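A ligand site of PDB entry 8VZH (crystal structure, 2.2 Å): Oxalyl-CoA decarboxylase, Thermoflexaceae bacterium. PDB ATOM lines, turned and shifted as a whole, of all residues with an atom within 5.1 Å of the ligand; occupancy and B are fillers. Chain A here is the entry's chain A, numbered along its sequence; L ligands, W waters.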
ATOM      1  N   ASN A  91       6.418 -10.831   5.105  1.00  0.00           N
ATOM      2  CA  ASN A  91       5.340 -11.282   4.239  1.00  0.00           C
ATOM      3  C   ASN A  91       5.354 -12.783   3.988  1.00  0.00           C
ATOM      4  O   ASN A  91       4.491 -13.276   3.249  1.00  0.00           O
ATOM      5  CB  ASN A  91       5.406 -10.547   2.893  1.00  0.00           C
ATOM      6  CG  ASN A  91       5.077  -9.082   3.023  1.00  0.00           C
ATOM      7  OD1 ASN A  91       3.943  -8.716   3.299  1.00  0.00           O
ATOM      8  ND2 ASN A  91       6.082  -8.234   2.838  1.00  0.00           N
ATOM      9  N   ASN A  92       6.294 -13.517   4.585  1.00  0.00           N
ATOM     10  CA  ASN A  92       6.487 -14.936   4.307  1.00  0.00           C
ATOM     11  C   ASN A  92       6.624 -15.196   2.806  1.00  0.00           C
ATOM     12  O   ASN A  92       5.889 -15.971   2.202  1.00  0.00           O
ATOM     13  CB  ASN A  92       5.353 -15.778   4.907  1.00  0.00           C
ATOM     14  CG  ASN A  92       5.161 -15.535   6.391  1.00  0.00           C
ATOM     15  OD1 ASN A  92       5.993 -15.917   7.206  1.00  0.00           O
ATOM     16  ND2 ASN A  92       4.052 -14.894   6.744  1.00  0.00           N
ATOM     17  N   ARG A 152       6.033 -22.718   5.742  1.00  0.00           N
ATOM     18  CA  ARG A 152       5.732 -21.297   5.621  1.00  0.00           C
ATOM     19  C   ARG A 152       6.863 -20.638   4.846  1.00  0.00           C
ATOM     20  O   ARG A 152       8.017 -20.673   5.309  1.00  0.00           O
ATOM     21  CB  ARG A 152       5.570 -20.661   6.994  1.00  0.00           C
ATOM     22  CG  ARG A 152       4.899 -19.309   6.962  1.00  0.00           C
ATOM     23  CD  ARG A 152       4.826 -18.688   8.361  1.00  0.00           C
ATOM     24  NE  ARG A 152       3.612 -17.902   8.523  1.00  0.00           N
ATOM     25  CZ  ARG A 152       3.308 -17.200   9.600  1.00  0.00           C
ATOM     26  NH1 ARG A 152       4.147 -17.079  10.617  1.00  0.00           N
ATOM     27  NH2 ARG A 152       2.123 -16.596   9.659  1.00  0.00           N
ATOM     28  N   PRO A 153       6.613 -20.060   3.679  1.00  0.00           N
ATOM     29  CA  PRO A 153       7.724 -19.570   2.855  1.00  0.00           C
ATOM     30  C   PRO A 153       8.467 -18.438   3.564  1.00  0.00           C
ATOM     31  O   PRO A 153       7.889 -17.701   4.366  1.00  0.00           O
ATOM     32  CB  PRO A 153       7.039 -19.088   1.578  1.00  0.00           C
ATOM     33  CG  PRO A 153       5.700 -19.815   1.562  1.00  0.00           C
ATOM     34  CD  PRO A 153       5.314 -19.931   3.005  1.00  0.00           C
ATOM     35  N   GLY A 211      -7.000 -13.354   1.629  1.00  0.00           N
ATOM     36  CA  GLY A 211      -5.712 -12.734   1.823  1.00  0.00           C
ATOM     37  C   GLY A 211      -4.680 -13.169   0.779  1.00  0.00           C
ATOM     38  O   GLY A 211      -4.941 -13.999  -0.086  1.00  0.00           O
ATOM     39  N   LYS A 212      -3.488 -12.577   0.891  1.00  0.00           N
ATOM     40  CA  LYS A 212      -2.469 -12.865  -0.117  1.00  0.00           C
ATOM     41  C   LYS A 212      -1.867 -14.262   0.042  1.00  0.00           C
ATOM     42  O   LYS A 212      -1.132 -14.706  -0.852  1.00  0.00           O
ATOM     43  CB  LYS A 212      -1.370 -11.796  -0.112  1.00  0.00           C
ATOM     44  CG  LYS A 212      -0.524 -11.659   1.143  1.00  0.00           C
ATOM     45  CD  LYS A 212       0.569 -10.620   0.874  1.00  0.00           C
ATOM     46  CE  LYS A 212       1.689 -10.625   1.907  1.00  0.00           C
ATOM     47  NZ  LYS A 212       1.328  -9.944   3.177  1.00  0.00           N
ATOM     48  N   GLY A 213      -2.159 -14.957   1.136  1.00  0.00           N
ATOM     49  CA  GLY A 213      -1.791 -16.366   1.219  1.00  0.00           C
ATOM     50  C   GLY A 213      -2.576 -17.205   0.233  1.00  0.00           C
ATOM     51  O   GLY A 213      -2.036 -18.140  -0.373  1.00  0.00           O
ATOM     52  N   TYR A 216      -0.906 -16.389  -3.035  1.00  0.00           N
ATOM     53  CA  TYR A 216       0.385 -17.062  -3.161  1.00  0.00           C
ATOM     54  C   TYR A 216       0.201 -18.552  -3.438  1.00  0.00           C
ATOM     55  O   TYR A 216       0.948 -19.143  -4.231  1.00  0.00           O
ATOM     56  CB  TYR A 216       1.230 -16.870  -1.903  1.00  0.00           C
ATOM     57  CG  TYR A 216       2.556 -17.615  -1.986  1.00  0.00           C
ATOM     58  CD1 TYR A 216       3.624 -17.088  -2.714  1.00  0.00           C
ATOM     59  CD2 TYR A 216       2.731 -18.856  -1.384  1.00  0.00           C
ATOM     60  CE1 TYR A 216       4.825 -17.767  -2.806  1.00  0.00           C
ATOM     61  CE2 TYR A 216       3.923 -19.539  -1.479  1.00  0.00           C
ATOM     62  CZ  TYR A 216       4.970 -18.995  -2.190  1.00  0.00           C
ATOM     63  OH  TYR A 216       6.162 -19.679  -2.284  1.00  0.00           O
ATOM     64  N   SER A 217      -0.789 -19.176  -2.796  1.00  0.00           N
ATOM     65  CA  SER A 217      -1.098 -20.581  -3.004  1.00  0.00           C
ATOM     66  C   SER A 217      -1.607 -20.881  -4.417  1.00  0.00           C
ATOM     67  O   SER A 217      -1.710 -22.060  -4.774  1.00  0.00           O
ATOM     68  CB  SER A 217      -2.139 -21.035  -1.973  1.00  0.00           C
ATOM     69  OG  SER A 217      -2.408 -22.422  -2.073  1.00  0.00           O
ATOM     70  N   SER A 237      -8.220  -8.634   1.051  1.00  0.00           N
ATOM     71  CA  SER A 237      -7.135  -7.837   1.610  1.00  0.00           C
ATOM     72  C   SER A 237      -6.430  -7.093   0.481  1.00  0.00           C
ATOM     73  O   SER A 237      -6.616  -7.421  -0.698  1.00  0.00           O
ATOM     74  CB  SER A 237      -6.141  -8.735   2.353  1.00  0.00           C
ATOM     75  OG  SER A 237      -5.316  -9.432   1.432  1.00  0.00           O
ATOM     76  N   MET A 239      -3.429  -7.059  -1.022  1.00  0.00           N
ATOM     77  CA  MET A 239      -2.853  -7.873  -2.072  1.00  0.00           C
ATOM     78  C   MET A 239      -3.644  -9.153  -2.330  1.00  0.00           C
ATOM     79  O   MET A 239      -3.306  -9.895  -3.253  1.00  0.00           O
ATOM     80  CB  MET A 239      -1.391  -8.188  -1.763  1.00  0.00           C
ATOM     81  CG  MET A 239      -0.510  -6.960  -1.960  1.00  0.00           C
ATOM     82  SD  MET A 239       1.249  -7.203  -1.639  1.00  0.00           S
ATOM     83  CE  MET A 239       1.612  -8.607  -2.687  1.00  0.00           C
ATOM     84  N   GLY A 240      -4.705  -9.402  -1.558  1.00  0.00           N
ATOM     85  CA  GLY A 240      -5.684 -10.396  -1.927  1.00  0.00           C
ATOM     86  C   GLY A 240      -6.622  -9.980  -3.042  1.00  0.00           C
ATOM     87  O   GLY A 240      -7.325 -10.832  -3.583  1.00  0.00           O
ATOM     88  N   GLY A 270      -6.010 -17.519   4.108  1.00  0.00           N
ATOM     89  CA  GLY A 270      -4.686 -16.973   3.888  1.00  0.00           C
ATOM     90  C   GLY A 270      -4.561 -15.525   4.293  1.00  0.00           C
ATOM     91  O   GLY A 270      -3.961 -14.721   3.565  1.00  0.00           O
ATOM     92  N   ALA A 271      -5.133 -15.154   5.436  1.00  0.00           N
ATOM     93  CA  ALA A 271      -5.024 -13.794   5.954  1.00  0.00           C
ATOM     94  C   ALA A 271      -4.792 -13.860   7.447  1.00  0.00           C
ATOM     95  O   ALA A 271      -5.306 -14.745   8.127  1.00  0.00           O
ATOM     96  CB  ALA A 271      -6.266 -12.956   5.643  1.00  0.00           C
ATOM     97  N   ARG A 272      -4.000 -12.923   7.964  1.00  0.00           N
ATOM     98  CA  ARG A 272      -3.646 -12.931   9.369  1.00  0.00           C
ATOM     99  C   ARG A 272      -4.485 -11.931  10.155  1.00  0.00           C
ATOM    100  O   ARG A 272      -4.880 -10.879   9.631  1.00  0.00           O
ATOM    101  CB  ARG A 272      -2.150 -12.627   9.571  1.00  0.00           C
ATOM    102  CG  ARG A 272      -1.247 -13.848   9.467  1.00  0.00           C
ATOM    103  CD  ARG A 272       0.224 -13.461   9.673  1.00  0.00           C
ATOM    104  NE  ARG A 272       0.682 -12.598   8.607  1.00  0.00           N
ATOM    105  CZ  ARG A 272       1.946 -12.250   8.397  1.00  0.00           C
ATOM    106  NH1 ARG A 272       2.922 -12.637   9.212  1.00  0.00           N
ATOM    107  NH2 ARG A 272       2.245 -11.509   7.337  1.00  0.00           N
ATOM    108  N   ASN A 274      -3.526  -9.718  12.076  1.00  0.00           N
ATOM    109  CA  ASN A 274      -2.474  -8.843  12.571  1.00  0.00           C
ATOM    110  C   ASN A 274      -2.950  -7.394  12.572  1.00  0.00           C
ATOM    111  O   ASN A 274      -4.150  -7.131  12.653  1.00  0.00           O
ATOM    112  CB  ASN A 274      -1.194  -9.011  11.731  1.00  0.00           C
ATOM    113  CG  ASN A 274      -1.421  -8.726  10.251  1.00  0.00           C
ATOM    114  OD1 ASN A 274      -2.540  -8.425   9.833  1.00  0.00           O
ATOM    115  ND2 ASN A 274      -0.362  -8.810   9.468  1.00  0.00           N
ATOM    116  N   MET A 276      -3.181  -5.246  10.216  1.00  0.00           N
ATOM    117  CA  MET A 276      -4.050  -4.888   9.099  1.00  0.00           C
ATOM    118  C   MET A 276      -5.512  -5.154   9.436  1.00  0.00           C
ATOM    119  O   MET A 276      -6.396  -4.380   9.050  1.00  0.00           O
ATOM    120  CB  MET A 276      -3.659  -5.646   7.840  1.00  0.00           C
ATOM    121  CG  MET A 276      -2.546  -4.995   7.062  1.00  0.00           C
ATOM    122  SD  MET A 276      -2.335  -5.651   5.390  1.00  0.00           S
ATOM    123  CE  MET A 276      -3.833  -6.623   5.238  1.00  0.00           C
ATOM    124  N   MET A 277      -5.783  -6.239  10.144  1.00  0.00           N
ATOM    125  CA  MET A 277      -7.135  -6.583  10.546  1.00  0.00           C
ATOM    126  C   MET A 277      -7.466  -6.079  11.945  1.00  0.00           C
ATOM    127  O   MET A 277      -8.445  -6.530  12.540  1.00  0.00           O
ATOM    128  CB  MET A 277      -7.332  -8.106  10.486  1.00  0.00           C
ATOM    129  CG  MET A 277      -7.151  -8.675   9.098  1.00  0.00           C
ATOM    130  SD  MET A 277      -8.299  -7.985   7.905  1.00  0.00           S
ATOM    131  CE  MET A 277      -7.487  -8.424   6.360  1.00  0.00           C
ATOM    132  N   MET A 294      -7.720 -20.506   7.926  1.00  0.00           N
ATOM    133  CA  MET A 294      -7.040 -21.371   6.974  1.00  0.00           C
ATOM    134  C   MET A 294      -5.648 -20.795   6.729  1.00  0.00           C
ATOM    135  O   MET A 294      -5.503 -19.705   6.168  1.00  0.00           O
ATOM    136  CB  MET A 294      -7.856 -21.458   5.678  1.00  0.00           C
ATOM    137  CG  MET A 294      -7.172 -22.176   4.534  1.00  0.00           C
ATOM    138  SD  MET A 294      -8.129 -21.987   2.999  1.00  0.00           S
ATOM    139  CE  MET A 294      -9.777 -22.428   3.572  1.00  0.00           C
ATOM    140  N   ASP A 295      -4.625 -21.511   7.189  1.00  0.00           N
ATOM    141  CA  ASP A 295      -3.258 -21.037   7.085  1.00  0.00           C
ATOM    142  C   ASP A 295      -2.339 -22.249   6.997  1.00  0.00           C
ATOM    143  O   ASP A 295      -2.600 -23.274   7.624  1.00  0.00           O
ATOM    144  CB  ASP A 295      -2.890 -20.153   8.279  1.00  0.00           C
ATOM    145  CG  ASP A 295      -1.743 -19.204   7.984  1.00  0.00           C
ATOM    146  OD1 ASP A 295      -0.607 -19.654   7.708  1.00  0.00           O
ATOM    147  OD2 ASP A 295      -1.983 -17.971   8.028  1.00  0.00           O
ATOM    148  N   ILE A 296      -1.263 -22.112   6.215  1.00  0.00           N
ATOM    149  CA  ILE A 296      -0.282 -23.196   6.152  1.00  0.00           C
ATOM    150  C   ILE A 296       0.519 -23.278   7.437  1.00  0.00           C
ATOM    151  O   ILE A 296       1.062 -24.341   7.768  1.00  0.00           O
ATOM    152  CB  ILE A 296       0.634 -23.015   4.921  1.00  0.00           C
ATOM    153  CG1 ILE A 296       1.350 -24.328   4.597  1.00  0.00           C
ATOM    154  CG2 ILE A 296       1.646 -21.884   5.149  1.00  0.00           C
ATOM    155  CD1 ILE A 296       2.242 -24.231   3.383  1.00  0.00           C
ATOM    156  N   SER A 297       0.568 -22.193   8.210  1.00  0.00           N
ATOM    157  CA  SER A 297       1.354 -22.136   9.438  1.00  0.00           C
ATOM    158  C   SER A 297       0.465 -22.491  10.622  1.00  0.00           C
ATOM    159  O   SER A 297      -0.427 -21.717  10.981  1.00  0.00           O
ATOM    160  CB  SER A 297       1.972 -20.752   9.623  1.00  0.00           C
ATOM    161  OG  SER A 297       2.553 -20.651  10.914  1.00  0.00           O
ATOM    162  N   GLU A 300       0.469 -19.862  13.510  1.00  0.00           N
ATOM    163  CA  GLU A 300      -0.348 -18.663  13.359  1.00  0.00           C
ATOM    164  C   GLU A 300      -1.772 -18.857  13.872  1.00  0.00           C
ATOM    165  O   GLU A 300      -2.450 -17.862  14.178  1.00  0.00           O
ATOM    166  CB  GLU A 300      -0.353 -18.253  11.879  1.00  0.00           C
ATOM    167  CG  GLU A 300      -0.984 -16.895  11.594  1.00  0.00           C
ATOM    168  CD  GLU A 300      -0.284 -15.770  12.317  1.00  0.00           C
ATOM    169  OE1 GLU A 300       0.965 -15.808  12.423  1.00  0.00           O
ATOM    170  OE2 GLU A 300      -0.976 -14.838  12.791  1.00  0.00           O
ATOM    171  N   GLY A 313      -3.076 -26.083   6.520  1.00  0.00           N
ATOM    172  CA  GLY A 313      -2.625 -26.712   5.300  1.00  0.00           C
ATOM    173  C   GLY A 313      -2.602 -25.699   4.170  1.00  0.00           C
ATOM    174  O   GLY A 313      -2.697 -24.489   4.390  1.00  0.00           O
ATOM    175  N   ASP A 314      -2.491 -26.224   2.952  1.00  0.00           N
ATOM    176  CA  ASP A 314      -2.415 -25.373   1.780  1.00  0.00           C
ATOM    177  C   ASP A 314      -3.800 -24.853   1.413  1.00  0.00           C
ATOM    178  O   ASP A 314      -4.788 -25.591   1.427  1.00  0.00           O
ATOM    179  CB  ASP A 314      -1.819 -26.154   0.601  1.00  0.00           C
ATOM    180  CG  ASP A 314      -1.842 -25.360  -0.688  1.00  0.00           C
ATOM    181  OD1 ASP A 314      -1.099 -24.352  -0.766  1.00  0.00           O
ATOM    182  OD2 ASP A 314      -2.590 -25.743  -1.600  1.00  0.00           O
ATOM    183  N   ALA A 315      -3.867 -23.558   1.075  1.00  0.00           N
ATOM    184  CA  ALA A 315      -5.149 -22.917   0.836  1.00  0.00           C
ATOM    185  C   ALA A 315      -5.847 -23.528  -0.382  1.00  0.00           C
ATOM    186  O   ALA A 315      -7.060 -23.762  -0.358  1.00  0.00           O
ATOM    187  CB  ALA A 315      -4.975 -21.414   0.632  1.00  0.00           C
ATOM    188  N   THR A 412       2.914  -6.267   4.397  1.00  0.00           N
ATOM    189  CA  THR A 412       2.758  -6.384   5.844  1.00  0.00           C
ATOM    190  C   THR A 412       3.700  -5.464   6.617  1.00  0.00           C
ATOM    191  O   THR A 412       3.327  -4.924   7.657  1.00  0.00           O
ATOM    192  CB  THR A 412       2.986  -7.839   6.278  1.00  0.00           C
ATOM    193  OG1 THR A 412       2.056  -8.700   5.612  1.00  0.00           O
ATOM    194  CG2 THR A 412       2.811  -7.986   7.781  1.00  0.00           C
HETATM  195  P1  LIG L   1      -2.873 -10.291   4.126  1.00  0.00           P
HETATM  196  O1  LIG L   1      -3.337 -10.376   2.691  1.00  0.00           O
HETATM  197  O2  LIG L   1      -1.814  -9.253   4.378  1.00  0.00           O
HETATM  198  O3  LIG L   1      -3.980 -10.301   5.160  1.00  0.00           O
HETATM  199  P2  LIG L   1      -0.968 -11.951   5.461  1.00  0.00           P
HETATM  200  O4  LIG L   1       0.364 -11.741   4.798  1.00  0.00           O
HETATM  201  O5  LIG L   1      -1.262 -11.238   6.772  1.00  0.00           O
HETATM  202  O6  LIG L   1      -2.137 -11.705   4.378  1.00  0.00           O
HETATM  203  O7  LIG L   1      -1.188 -13.511   5.754  1.00  0.00           O
HETATM  204  C1  LIG L   1      -0.935 -14.491   4.753  1.00  0.00           C
HETATM  205  C2  LIG L   1      -0.878 -15.844   5.426  1.00  0.00           C
HETATM  206  O8  LIG L   1      -0.922 -16.848   4.423  1.00  0.00           O
HETATM  207  C3  LIG L   1       0.402 -16.078   6.212  1.00  0.00           C
HETATM  208  O9  LIG L   1       0.054 -16.283   7.583  1.00  0.00           O
HETATM  209  C4  LIG L   1       1.005 -17.360   5.639  1.00  0.00           C
HETATM  210  O10 LIG L   1       1.447 -18.255   6.652  1.00  0.00           O
HETATM  211  C5  LIG L   1      -0.172 -17.963   4.887  1.00  0.00           C
HETATM  212  N1  LIG L   1       0.219 -18.819   3.745  1.00  0.00           N
HETATM  213  C6  LIG L   1       1.349 -18.734   3.028  1.00  0.00           C
HETATM  214  N2  LIG L   1       1.366 -19.680   2.048  1.00  0.00           N
HETATM  215  C7  LIG L   1       0.229 -20.387   2.145  1.00  0.00           C
HETATM  216  C8  LIG L   1      -0.389 -21.525   1.427  1.00  0.00           C
HETATM  217  N3  LIG L   1       0.237 -22.119   0.385  1.00  0.00           N
HETATM  218  N4  LIG L   1      -1.600 -21.955   1.856  1.00  0.00           N
HETATM  219  C9  LIG L   1      -2.240 -21.376   2.889  1.00  0.00           C
HETATM  220  N5  LIG L   1      -1.731 -20.337   3.587  1.00  0.00           N
HETATM  221  C10 LIG L   1      -0.522 -19.814   3.265  1.00  0.00           C
HETATM  222  O   HOH W   1      -0.484  -8.624   6.664  1.00  0.00           O
HETATM  223  O   HOH W   2      -3.873  -9.424   7.633  1.00  0.00           O
HETATM  224  O   HOH W   3       2.259 -13.805   4.810  1.00  0.00           O
HETATM  225  O   HOH W   4       3.096 -22.930  -0.474  1.00  0.00           O
HETATM  226  O   HOH W   5      -2.667  -7.946   1.490  1.00  0.00           O
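Water W2 lies within hydrogen-bond range of an oxygen (O3) of the ligand, the backbone carbonyl oxygen of Arg 272 and the side-chain amide oxygen of Asn 274. Water W1 lies within hydrogen-bond range of an oxygen (O2) of the ligand (2.7 Å), the side-chain hydroxyl of Thr 412 (2.8 Å), the side-chain amide nitrogen of Asn 274 (2.8 Å) and the side-chain sulfur of Met 276 (3.7 Å). Water W5 lies within hydrogen-bond range of the backbone NH (N) of Met 239 (2.8 Å), an oxygen (O1) of the ligand (2.8 Å) and the side-chain hydroxyl (OG) of Ser 237 (3.0 Å). Water W3 lies within hydrogen-bond range of O of Asn 91 (2.8 Å), O4 of the ligand (2.8 Å), ND2 of Asn 92 (2.9 Å) and NH2 of Arg 272 (3.4 Å).
The backbone NH of Lys 212 lies within hydrogen-bond range of the backbone carbonyl oxygen of Gly 270, 3.5 Å away. The side-chain hydroxyl (OG) of Ser 217 sits at hydrogen-bond distance from the side-chain carboxylate (OD1) of Asp 314 (2.7 Å). The side-chain amide oxygen (OD1) of Asn 92 sits close to the guanidinium group (NE) of Arg 152 (3.4 Å). NH2 of Arg 272 is in hydrogen-bond range of OG1 of Thr 412 (3.3 Å). O of Arg 272 sits close to OD1 of Asn 274 (3.4 Å). The backbone NH (N) of Met 276 lies close to the side-chain amide oxygen (OD1) of Asn 274 (3.3 Å). OD1 of Asn 91 sits at hydrogen-bond distance from N of Thr 412 (2.9 Å). The backbone NH (N) of Glu 300 is in hydrogen-bond range of the side-chain hydroxyl (OG) of Ser 297 (3.4 Å).
OG of Ser 237 is in hydrogen-bond range of O1 of the ligand, 2.5 Å away. N of Lys 212 is in hydrogen-bond range of O1 of the ligand (2.8 Å). The side-chain amino group of Lys 212 is in salt-bridge range of an oxygen (O4) of the ligand (2.6 Å). O9 of the ligand lies within hydrogen-bond range of OD2 of Asp 295. OD1 of Asp 314 is in hydrogen-bond range of N3 of the ligand. An oxygen (O10) of the ligand lies within hydrogen-bond range of the guanidinium group of Arg 152 (2.9 Å). The backbone NH (N) of Ala 315 lies within hydrogen-bond range of a nitrogen (N4) of the ligand, 2.9 Å away. N of Arg 272 lies close to O5 of the ligand (3.4 Å). An oxygen (O5) of the ligand is in salt-bridge range of the guanidinium group (NE) of Arg 272, 3.0 Å away. A nitrogen (N5) of the ligand is in hydrogen-bond range of the backbone NH (N) of Ile 296 (3.2 Å).
An oxygen (O2) of the ligand sits close to the side-chain sulfur (SD) of Met 276 (3.8 Å). ND2 of Asn 92 touches C3 of the ligand, at 3.9 Å. Gly 211 touches the ligand (CA to O1, 3.5 Å). Gly 213 touches the ligand (CA to O8, 3.4 Å). CD2 of Tyr 216 touches N2 of the ligand, 3.8 Å away. Ser 217 touches the ligand (CB to N3, 3.5 Å). Gly 270 touches the ligand (O to C1, 3.3 Å). Ala 271 touches the ligand. Asn 274 touches the ligand (ND2 to O5, 3.7 Å). Ser 297 touches the ligand. O of Gly 313 touches C9 of the ligand, 3.5 Å away. Thr 412 touches the ligand. Hydrophobic or aromatic side chains within 4 Å of the ligand: Tyr 216, Ala 271, Met 276, Ile 296 and Ala 315. The nearest printed residue that does not touch the ligand is Pro 153 (4.1 Å).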
